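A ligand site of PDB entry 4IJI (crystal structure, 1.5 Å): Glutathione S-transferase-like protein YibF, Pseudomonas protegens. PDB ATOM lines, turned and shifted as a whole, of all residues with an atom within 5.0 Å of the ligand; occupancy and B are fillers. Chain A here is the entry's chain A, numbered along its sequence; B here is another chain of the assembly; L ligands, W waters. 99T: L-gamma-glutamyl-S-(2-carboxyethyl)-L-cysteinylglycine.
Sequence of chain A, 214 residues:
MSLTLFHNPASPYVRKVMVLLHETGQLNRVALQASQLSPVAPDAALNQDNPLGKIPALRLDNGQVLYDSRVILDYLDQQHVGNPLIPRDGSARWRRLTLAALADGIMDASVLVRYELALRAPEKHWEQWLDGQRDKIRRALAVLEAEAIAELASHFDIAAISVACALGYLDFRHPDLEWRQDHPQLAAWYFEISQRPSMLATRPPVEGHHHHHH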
ATOM      1  N   ALA A  10       6.362  10.553  -9.324  1.00  0.00           N
ATOM      2  CA  ALA A  10       7.420   9.715  -9.907  1.00  0.00           C
ATOM      3  C   ALA A  10       8.482  10.517 -10.667  1.00  0.00           C
ATOM      4  O   ALA A  10       9.655  10.148 -10.709  1.00  0.00           O
ATOM      5  CB  ALA A  10       6.807   8.635 -10.800  1.00  0.00           C
ATOM      6  N   SER A  11       8.062  11.613 -11.291  1.00  0.00           N
ATOM      7  CA  SER A  11       8.949  12.321 -12.198  1.00  0.00           C
ATOM      8  C   SER A  11      10.070  13.068 -11.482  1.00  0.00           C
ATOM      9  O   SER A  11       9.802  13.919 -10.621  1.00  0.00           O
ATOM     10  CB  SER A  11       8.145  13.311 -13.064  1.00  0.00           C
ATOM     11  OG  SER A  11       9.042  14.106 -13.834  1.00  0.00           O
ATOM     12  N   PRO A  12      11.328  12.790 -11.854  1.00  0.00           N
ATOM     13  CA  PRO A  12      12.432  13.498 -11.193  1.00  0.00           C
ATOM     14  C   PRO A  12      12.578  14.938 -11.686  1.00  0.00           C
ATOM     15  O   PRO A  12      13.184  15.748 -10.990  1.00  0.00           O
ATOM     16  CB  PRO A  12      13.660  12.654 -11.568  1.00  0.00           C
ATOM     17  CG  PRO A  12      13.295  12.078 -12.920  1.00  0.00           C
ATOM     18  CD  PRO A  12      11.806  11.835 -12.878  1.00  0.00           C
ATOM     19  N   TYR A  13      12.057  15.252 -12.871  1.00  0.00           N
ATOM     20  CA  TYR A  13      12.078  16.630 -13.347  1.00  0.00           C
ATOM     21  C   TYR A  13      11.052  17.458 -12.577  1.00  0.00           C
ATOM     22  O   TYR A  13      11.306  18.597 -12.215  1.00  0.00           O
ATOM     23  CB  TYR A  13      11.776  16.696 -14.836  1.00  0.00           C
ATOM     24  CG  TYR A  13      12.611  15.773 -15.684  1.00  0.00           C
ATOM     25  CD1 TYR A  13      13.851  16.156 -16.171  1.00  0.00           C
ATOM     26  CD2 TYR A  13      12.145  14.496 -15.999  1.00  0.00           C
ATOM     27  CE1 TYR A  13      14.608  15.305 -16.972  1.00  0.00           C
ATOM     28  CE2 TYR A  13      12.899  13.628 -16.787  1.00  0.00           C
ATOM     29  CZ  TYR A  13      14.118  14.050 -17.257  1.00  0.00           C
ATOM     30  OH  TYR A  13      14.859  13.203 -18.043  1.00  0.00           O
ATOM     31  N   LYS A  16      12.621  18.160  -9.113  1.00  0.00           N
ATOM     32  CA  LYS A  16      13.513  19.313  -9.025  1.00  0.00           C
ATOM     33  C   LYS A  16      12.731  20.580  -8.717  1.00  0.00           C
ATOM     34  O   LYS A  16      13.138  21.394  -7.890  1.00  0.00           O
ATOM     35  CB  LYS A  16      14.270  19.559 -10.347  1.00  0.00           C
ATOM     36  CG  LYS A  16      15.296  18.530 -10.720  1.00  0.00           C
ATOM     37  CD  LYS A  16      16.094  19.003 -11.938  1.00  0.00           C
ATOM     38  CE  LYS A  16      15.237  19.005 -13.206  1.00  0.00           C
ATOM     39  NZ  LYS A  16      16.018  19.483 -14.385  1.00  0.00           N
ATOM     40  N   LEU A  37       1.019   9.751 -17.453  1.00  0.00           N
ATOM     41  CA  LEU A  37       1.309   9.885 -18.873  1.00  0.00           C
ATOM     42  C   LEU A  37       2.525   9.071 -19.292  1.00  0.00           C
ATOM     43  O   LEU A  37       3.357   8.707 -18.465  1.00  0.00           O
ATOM     44  CB  LEU A  37       1.556  11.361 -19.207  1.00  0.00           C
ATOM     45  CG  LEU A  37       2.944  11.910 -18.844  1.00  0.00           C
ATOM     46  CD1 LEU A  37       3.105  13.306 -19.399  1.00  0.00           C
ATOM     47  CD2 LEU A  37       3.232  11.907 -17.345  1.00  0.00           C
ATOM     48  N   SER A  38       2.628   8.805 -20.586  1.00  0.00           N
ATOM     49  CA  SER A  38       3.833   8.216 -21.175  1.00  0.00           C
ATOM     50  C   SER A  38       3.767   8.533 -22.660  1.00  0.00           C
ATOM     51  O   SER A  38       2.757   9.040 -23.119  1.00  0.00           O
ATOM     52  CB  SER A  38       3.891   6.703 -20.930  1.00  0.00           C
ATOM     53  OG  SER A  38       3.175   6.028 -21.943  1.00  0.00           O
ATOM     54  N   PRO A  39       4.862   8.270 -23.413  1.00  0.00           N
ATOM     55  CA  PRO A  39       4.780   8.552 -24.843  1.00  0.00           C
ATOM     56  C   PRO A  39       3.712   7.748 -25.585  1.00  0.00           C
ATOM     57  O   PRO A  39       3.285   8.179 -26.654  1.00  0.00           O
ATOM     58  CB  PRO A  39       6.185   8.179 -25.342  1.00  0.00           C
ATOM     59  CG  PRO A  39       7.069   8.443 -24.160  1.00  0.00           C
ATOM     60  CD  PRO A  39       6.240   7.979 -22.989  1.00  0.00           C
ATOM     61  N   LEU A  52       4.456  19.090 -26.193  1.00  0.00           N
ATOM     62  CA  LEU A  52       5.395  17.969 -26.133  1.00  0.00           C
ATOM     63  C   LEU A  52       4.893  16.804 -25.289  1.00  0.00           C
ATOM     64  O   LEU A  52       5.464  15.720 -25.325  1.00  0.00           O
ATOM     65  CB  LEU A  52       6.746  18.441 -25.590  1.00  0.00           C
ATOM     66  CG  LEU A  52       7.434  19.566 -26.333  1.00  0.00           C
ATOM     67  CD1 LEU A  52       8.661  19.992 -25.543  1.00  0.00           C
ATOM     68  CD2 LEU A  52       7.847  19.108 -27.732  1.00  0.00           C
ATOM     69  N   GLY A  53       3.837  17.026 -24.506  1.00  0.00           N
ATOM     70  CA  GLY A  53       3.299  15.966 -23.689  1.00  0.00           C
ATOM     71  C   GLY A  53       4.264  15.524 -22.606  1.00  0.00           C
ATOM     72  O   GLY A  53       4.409  14.335 -22.328  1.00  0.00           O
ATOM     73  N   LYS A  54       4.935  16.487 -21.963  1.00  0.00           N
ATOM     74  CA  LYS A  54       5.844  16.151 -20.875  1.00  0.00           C
ATOM     75  C   LYS A  54       5.581  17.008 -19.642  1.00  0.00           C
ATOM     76  O   LYS A  54       5.159  18.154 -19.758  1.00  0.00           O
ATOM     77  CB  LYS A  54       7.320  16.271 -21.294  1.00  0.00           C
ATOM     78  CG  LYS A  54       7.750  15.287 -22.397  1.00  0.00           C
ATOM     79  CD  LYS A  54       9.267  15.288 -22.590  1.00  0.00           C
ATOM     80  CE  LYS A  54       9.686  14.304 -23.664  1.00  0.00           C
ATOM     81  NZ  LYS A  54      11.171  14.166 -23.685  1.00  0.00           N
ATOM     82  N   ILE A  55       5.871  16.452 -18.468  1.00  0.00           N
ATOM     83  CA  ILE A  55       5.818  17.218 -17.231  1.00  0.00           C
ATOM     84  C   ILE A  55       7.236  17.374 -16.684  1.00  0.00           C
ATOM     85  O   ILE A  55       8.099  16.515 -16.916  1.00  0.00           O
ATOM     86  CB  ILE A  55       4.899  16.541 -16.172  1.00  0.00           C
ATOM     87  CG1 ILE A  55       5.420  15.173 -15.775  1.00  0.00           C
ATOM     88  CG2 ILE A  55       3.469  16.473 -16.690  1.00  0.00           C
ATOM     89  CD1 ILE A  55       4.511  14.495 -14.744  1.00  0.00           C
ATOM     90  N   PRO A  56       7.504  18.461 -15.948  1.00  0.00           N
ATOM     91  CA  PRO A  56       6.582  19.514 -15.521  1.00  0.00           C
ATOM     92  C   PRO A  56       6.226  20.520 -16.619  1.00  0.00           C
ATOM     93  O   PRO A  56       6.977  20.740 -17.578  1.00  0.00           O
ATOM     94  CB  PRO A  56       7.370  20.233 -14.421  1.00  0.00           C
ATOM     95  CG  PRO A  56       8.805  20.046 -14.835  1.00  0.00           C
ATOM     96  CD  PRO A  56       8.857  18.647 -15.391  1.00  0.00           C
ATOM     97  N   ASP A  68      10.575  23.608 -20.526  1.00  0.00           N
ATOM     98  CA  ASP A  68      10.550  22.414 -19.663  1.00  0.00           C
ATOM     99  C   ASP A  68      11.049  22.745 -18.251  1.00  0.00           C
ATOM    100  O   ASP A  68      10.978  23.910 -17.825  1.00  0.00           O
ATOM    101  CB  ASP A  68      11.403  21.311 -20.311  1.00  0.00           C
ATOM    102  CG  ASP A  68      12.877  21.679 -20.401  1.00  0.00           C
ATOM    103  OD1 ASP A  68      13.221  22.855 -20.156  1.00  0.00           O
ATOM    104  OD2 ASP A  68      13.692  20.777 -20.715  1.00  0.00           O
ATOM    105  N   SER A  69      11.520  21.744 -17.519  1.00  0.00           N
ATOM    106  CA  SER A  69      11.858  21.960 -16.116  1.00  0.00           C
ATOM    107  C   SER A  69      12.894  23.058 -15.904  1.00  0.00           C
ATOM    108  O   SER A  69      12.803  23.793 -14.938  1.00  0.00           O
ATOM    109  CB  SER A  69      12.299  20.663 -15.430  1.00  0.00           C
ATOM    110  OG  SER A  69      13.562  20.224 -15.928  1.00  0.00           O
ATOM    111  N   ARG A  70      13.886  23.171 -16.783  1.00  0.00           N
ATOM    112  CA  ARG A  70      14.909  24.191 -16.549  1.00  0.00           C
ATOM    113  C   ARG A  70      14.336  25.595 -16.654  1.00  0.00           C
ATOM    114  O   ARG A  70      14.741  26.493 -15.911  1.00  0.00           O
ATOM    115  CB  ARG A  70      16.069  24.061 -17.530  1.00  0.00           C
ATOM    116  CG  ARG A  70      16.772  22.748 -17.478  1.00  0.00           C
ATOM    117  CD  ARG A  70      18.021  22.844 -18.344  1.00  0.00           C
ATOM    118  NE  ARG A  70      18.479  21.545 -18.825  1.00  0.00           N
ATOM    119  CZ  ARG A  70      19.424  21.419 -19.745  1.00  0.00           C
ATOM    120  NH1 ARG A  70      20.011  22.513 -20.234  1.00  0.00           N
ATOM    121  NH2 ARG A  70      19.822  20.205 -20.130  1.00  0.00           N
ATOM    122  N   VAL A 111      15.306   7.721 -17.837  1.00  0.00           N
ATOM    123  CA  VAL A 111      13.927   7.699 -18.290  1.00  0.00           C
ATOM    124  C   VAL A 111      13.768   6.879 -19.565  1.00  0.00           C
ATOM    125  O   VAL A 111      12.841   6.069 -19.674  1.00  0.00           O
ATOM    126  CB  VAL A 111      13.393   9.144 -18.473  1.00  0.00           C
ATOM    127  CG1 VAL A 111      12.056   9.139 -19.228  1.00  0.00           C
ATOM    128  CG2 VAL A 111      13.252   9.806 -17.110  1.00  0.00           C
ATOM    129  N   ARG A 114      13.928   3.324 -18.493  1.00  0.00           N
ATOM    130  CA  ARG A 114      12.644   2.958 -17.892  1.00  0.00           C
ATOM    131  C   ARG A 114      11.599   2.630 -18.956  1.00  0.00           C
ATOM    132  O   ARG A 114      10.901   1.628 -18.856  1.00  0.00           O
ATOM    133  CB  ARG A 114      12.133   4.092 -16.999  1.00  0.00           C
ATOM    134  CG  ARG A 114      10.671   3.944 -16.553  1.00  0.00           C
ATOM    135  CD  ARG A 114      10.443   2.697 -15.731  1.00  0.00           C
ATOM    136  NE  ARG A 114       9.038   2.555 -15.331  1.00  0.00           N
ATOM    137  CZ  ARG A 114       8.608   1.642 -14.461  1.00  0.00           C
ATOM    138  NH1 ARG A 114       9.475   0.808 -13.903  1.00  0.00           N
ATOM    139  NH2 ARG A 114       7.325   1.541 -14.151  1.00  0.00           N
ATOM    140  N   TYR A 115      11.491   3.468 -19.981  1.00  0.00           N
ATOM    141  CA  TYR A 115      10.462   3.253 -20.992  1.00  0.00           C
ATOM    142  C   TYR A 115      10.775   1.982 -21.804  1.00  0.00           C
ATOM    143  O   TYR A 115       9.857   1.216 -22.150  1.00  0.00           O
ATOM    144  CB  TYR A 115      10.319   4.472 -21.912  1.00  0.00           C
ATOM    145  CG  TYR A 115       9.671   5.691 -21.281  1.00  0.00           C
ATOM    146  CD1 TYR A 115       8.748   5.571 -20.253  1.00  0.00           C
ATOM    147  CD2 TYR A 115       9.974   6.965 -21.739  1.00  0.00           C
ATOM    148  CE1 TYR A 115       8.142   6.691 -19.689  1.00  0.00           C
ATOM    149  CE2 TYR A 115       9.379   8.092 -21.171  1.00  0.00           C
ATOM    150  CZ  TYR A 115       8.478   7.953 -20.149  1.00  0.00           C
ATOM    151  OH  TYR A 115       7.888   9.070 -19.600  1.00  0.00           O
ATOM    152  N   TYR A 169      16.066   9.024  -8.534  1.00  0.00           N
ATOM    153  CA  TYR A 169      15.366   8.362  -9.637  1.00  0.00           C
ATOM    154  C   TYR A 169      16.017   7.040  -9.994  1.00  0.00           C
ATOM    155  O   TYR A 169      15.310   6.072 -10.319  1.00  0.00           O
ATOM    156  CB  TYR A 169      15.266   9.279 -10.860  1.00  0.00           C
ATOM    157  CG  TYR A 169      14.396   8.732 -11.970  1.00  0.00           C
ATOM    158  CD1 TYR A 169      12.999   8.700 -11.841  1.00  0.00           C
ATOM    159  CD2 TYR A 169      14.948   8.232 -13.140  1.00  0.00           C
ATOM    160  CE1 TYR A 169      12.191   8.208 -12.858  1.00  0.00           C
ATOM    161  CE2 TYR A 169      14.162   7.721 -14.162  1.00  0.00           C
ATOM    162  CZ  TYR A 169      12.788   7.703 -14.024  1.00  0.00           C
ATOM    163  OH  TYR A 169      12.005   7.197 -15.038  1.00  0.00           O
ATOM    164  N   PHE A 172      14.805   4.610  -7.466  1.00  0.00           N
ATOM    165  CA  PHE A 172      13.373   4.386  -7.632  1.00  0.00           C
ATOM    166  C   PHE A 172      13.061   3.457  -8.809  1.00  0.00           C
ATOM    167  O   PHE A 172      12.393   2.435  -8.639  1.00  0.00           O
ATOM    168  CB  PHE A 172      12.682   5.762  -7.770  1.00  0.00           C
ATOM    169  CG  PHE A 172      11.230   5.704  -8.175  1.00  0.00           C
ATOM    170  CD1 PHE A 172      10.320   4.913  -7.493  1.00  0.00           C
ATOM    171  CD2 PHE A 172      10.773   6.478  -9.228  1.00  0.00           C
ATOM    172  CE1 PHE A 172       8.973   4.891  -7.866  1.00  0.00           C
ATOM    173  CE2 PHE A 172       9.435   6.457  -9.605  1.00  0.00           C
ATOM    174  CZ  PHE A 172       8.537   5.659  -8.921  1.00  0.00           C
ATOM    175  N   ARG A 173      13.540   3.799 -10.004  1.00  0.00           N
ATOM    176  CA  ARG A 173      13.216   3.047 -11.205  1.00  0.00           C
ATOM    177  C   ARG A 173      14.233   1.953 -11.516  1.00  0.00           C
ATOM    178  O   ARG A 173      13.904   0.964 -12.152  1.00  0.00           O
ATOM    179  CB  ARG A 173      13.088   3.961 -12.416  1.00  0.00           C
ATOM    180  CG  ARG A 173      11.841   4.846 -12.407  1.00  0.00           C
ATOM    181  CD  ARG A 173      10.567   4.056 -12.124  1.00  0.00           C
ATOM    182  NE  ARG A 173       9.397   4.841 -12.533  1.00  0.00           N
ATOM    183  CZ  ARG A 173       8.138   4.555 -12.199  1.00  0.00           C
ATOM    184  NH1 ARG A 173       7.874   3.490 -11.459  1.00  0.00           N
ATOM    185  NH2 ARG A 173       7.159   5.331 -12.620  1.00  0.00           N
ATOM    186  N   ARG B  70      21.954  24.361 -24.279  1.00  0.00           N
ATOM    187  CA  ARG B  70      21.278  25.507 -23.688  1.00  0.00           C
ATOM    188  C   ARG B  70      22.185  26.317 -22.776  1.00  0.00           C
ATOM    189  O   ARG B  70      22.132  27.540 -22.752  1.00  0.00           O
ATOM    190  CB  ARG B  70      20.011  25.077 -22.957  1.00  0.00           C
ATOM    191  CG  ARG B  70      18.889  24.739 -23.891  1.00  0.00           C
ATOM    192  CD  ARG B  70      17.589  24.740 -23.118  1.00  0.00           C
ATOM    193  NE  ARG B  70      16.947  23.428 -23.178  1.00  0.00           N
ATOM    194  CZ  ARG B  70      15.864  23.093 -22.468  1.00  0.00           C
ATOM    195  NH1 ARG B  70      15.316  23.960 -21.626  1.00  0.00           N
ATOM    196  NH2 ARG B  70      15.360  21.873 -22.584  1.00  0.00           N
ATOM    197  N   LYS B 136       4.212  14.170 -30.955  1.00  0.00           N
ATOM    198  CA  LYS B 136       4.783  15.305 -30.229  1.00  0.00           C
ATOM    199  C   LYS B 136       5.204  16.384 -31.227  1.00  0.00           C
ATOM    200  O   LYS B 136       4.945  17.578 -31.021  1.00  0.00           O
ATOM    201  CB  LYS B 136       6.013  14.883 -29.402  1.00  0.00           C
ATOM    202  CG  LYS B 136       5.692  13.928 -28.243  1.00  0.00           C
ATOM    203  CD  LYS B 136       6.978  13.659 -27.441  1.00  0.00           C
ATOM    204  CE  LYS B 136       6.801  12.510 -26.427  1.00  0.00           C
ATOM    205  NZ  LYS B 136       5.794  12.876 -25.357  1.00  0.00           N
HETATM  206  O32 99T L   1       5.598  11.350 -23.231  1.00  0.00           O
HETATM  207  C3  99T L   1       6.521  11.531 -22.392  1.00  0.00           C
HETATM  208  O31 99T L   1       7.724  11.522 -22.752  1.00  0.00           O
HETATM  209  CA3 99T L   1       6.179  11.759 -20.950  1.00  0.00           C
HETATM  210  N3  99T L   1       7.290  11.764 -20.053  1.00  0.00           N
HETATM  211  C2  99T L   1       7.491  12.799 -19.120  1.00  0.00           C
HETATM  212  O2  99T L   1       6.704  13.745 -19.075  1.00  0.00           O
HETATM  213  CA2 99T L   1       8.680  12.727 -18.216  1.00  0.00           C
HETATM  214  CB2 99T L   1       8.304  12.107 -16.915  1.00  0.00           C
HETATM  215  SG2 99T L   1       9.657  11.603 -15.914  1.00  0.00           S
HETATM  216  N2  99T L   1       9.160  14.066 -18.090  1.00  0.00           N
HETATM  217  CD1 99T L   1      10.242  14.471 -18.888  1.00  0.00           C
HETATM  218  OE1 99T L   1      10.781  13.685 -19.671  1.00  0.00           O
HETATM  219  CG1 99T L   1      10.698  15.883 -18.769  1.00  0.00           C
HETATM  220  CB1 99T L   1      11.889  16.280 -19.568  1.00  0.00           C
HETATM  221  CA1 99T L   1      11.997  17.751 -19.844  1.00  0.00           C
HETATM  222  N1  99T L   1      13.160  17.977 -20.664  1.00  0.00           N
HETATM  223  C1  99T L   1      12.212  18.481 -18.571  1.00  0.00           C
HETATM  224  O01 99T L   1      13.378  18.739 -18.162  1.00  0.00           O
HETATM  225  O02 99T L   1      11.205  18.870 -17.909  1.00  0.00           O
HETATM  226  C08 99T L   1       9.186  10.150 -15.038  1.00  0.00           C
HETATM  227  C09 99T L   1       9.109   8.863 -15.775  1.00  0.00           C
HETATM  228  C10 99T L   1       8.688   7.732 -14.904  1.00  0.00           C
HETATM  229  O11 99T L   1       7.456   7.567 -14.651  1.00  0.00           O
HETATM  230  O12 99T L   1       9.559   7.001 -14.383  1.00  0.00           O
HETATM  231  O   HOH W   1       9.494  10.739 -24.784  1.00  0.00           O
HETATM  232  O   HOH W   2      13.332  13.156 -20.838  1.00  0.00           O
HETATM  233  O   HOH W   3      15.725  16.851 -20.027  1.00  0.00           O
HETATM  234  O   HOH W   4      16.113  18.822 -17.848  1.00  0.00           O
HETATM  235  O   HOH W   5      11.190  18.610 -22.993  1.00  0.00           O
HETATM  236  O   HOH W   6       5.575   9.422 -14.999  1.00  0.00           O
HETATM  237  O   HOH W   7       2.848  12.002 -23.296  1.00  0.00           O
HETATM  238  O   HOH W   8       8.744  19.275 -19.172  1.00  0.00           O
HETATM  239  O   HOH W   9      10.195  11.757 -21.596  1.00  0.00           O
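The side-chain hydroxyl (OG) of Ser 11 lies close to the backbone NH (N) of Tyr 13, 3.4 Å away.
OD2 of Asp 68 is in salt-bridge range of NH2 of Arg 70 of chain B.
The side-chain carboxylate of Asp 68 lies close to the backbone NH of Arg 70 of chain A (3.5 Å).
OG of Ser 69 lies within hydrogen-bond range of NZ of Lys 16 (3.0 Å).
The side-chain amino group (NZ) of Lys 136 of chain B is in hydrogen-bond range of the backbone carbonyl oxygen (O) of Leu 52, 2.9 Å away.
N2 of the ligand sits at hydrogen-bond distance from O of Ile 55.
A nitrogen (N3) of the ligand is in hydrogen-bond range of the side-chain hydroxyl of Tyr 115, 2.8 Å away.
The side-chain hydroxyl (OH) of Tyr 169 sits at hydrogen-bond distance from an oxygen (O12) of the ligand, at 2.5 Å.
The side-chain carboxylate of Asp 68 lies within salt-bridge range of a nitrogen (N1) of the ligand, 2.9 Å away.
NZ of Lys 136 of chain B is in salt-bridge range of O32 of the ligand (2.6 Å).
NE of Arg 173 lies within salt-bridge range of O12 of the ligand.
N of Ile 55 is in hydrogen-bond range of O2 of the ligand (2.9 Å).
OG of Ser 69 is in hydrogen-bond range of O01 of the ligand (2.7 Å).
OG of Ser 11 sits close to SG2 of the ligand, at 3.3 Å.
O02 of the ligand lies within hydrogen-bond range of N of Ser 69 (2.9 Å).
An oxygen (O32) of the ligand lies close to the backbone nitrogen of Pro 39 (3.2 Å).
O of Gly 53 lies close to O32 of the ligand, at 3.3 Å.
CD of Pro 12 touches SG2 of the ligand (3.7 Å).
CD1 of Tyr 13 touches O01 of the ligand (3.3 Å).
CD1 of Leu 37 touches O2 of the ligand, at 3.6 Å.
Ser 38 touches the ligand.
Lys 54 touches the ligand.
Pro 56 touches the ligand (CD to O02, 3.5 Å).
Arg 114 touches the ligand (CG to O12, 3.9 Å).
Hydrophobic or aromatic side chains within 4 Å of the ligand: Pro 12, Tyr 13, Leu 37, Pro 39, Ile 55, Pro 56, Tyr 115 and Tyr 169.
17 residues have an atom within 4 Å of the ligand: Ser 11, Pro 12, Tyr 13, Leu 37, Ser 38, Pro 39, Gly 53, Lys 54, Ile 55, Pro 56, Asp 68, Ser 69, Arg 114, Tyr 115, Tyr 169, Arg 173 and Lys 136 of chain B.
Along chain A the residues within 4 Å of the ligand span positions 11 to 173.
The nearest printed residue that does not touch the ligand is Ala 10 (4.05 Å).
Water W9 bridges O31 of the ligand (2.7 Å) and NZ of Lys 54 (3.3 Å).
Water W4 lies within hydrogen-bond range of O01 of the ligand (2.8 Å) and OG of Ser 69 (3.5 Å).
Water W8 lies within hydrogen-bond range of O of Pro 56 (2.8 Å) and O02 of the ligand (2.8 Å).
Water W7 lies within hydrogen-bond range of an oxygen (O32) of the ligand (2.8 Å), the backbone carbonyl oxygen (O) of Ser 38 (3.0 Å) and the backbone carbonyl oxygen (O) of Gly 53 (3.0 Å).
Water W2 bridges OE1 of the ligand (2.9 Å) and OH of Tyr 13 (3.2 Å).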
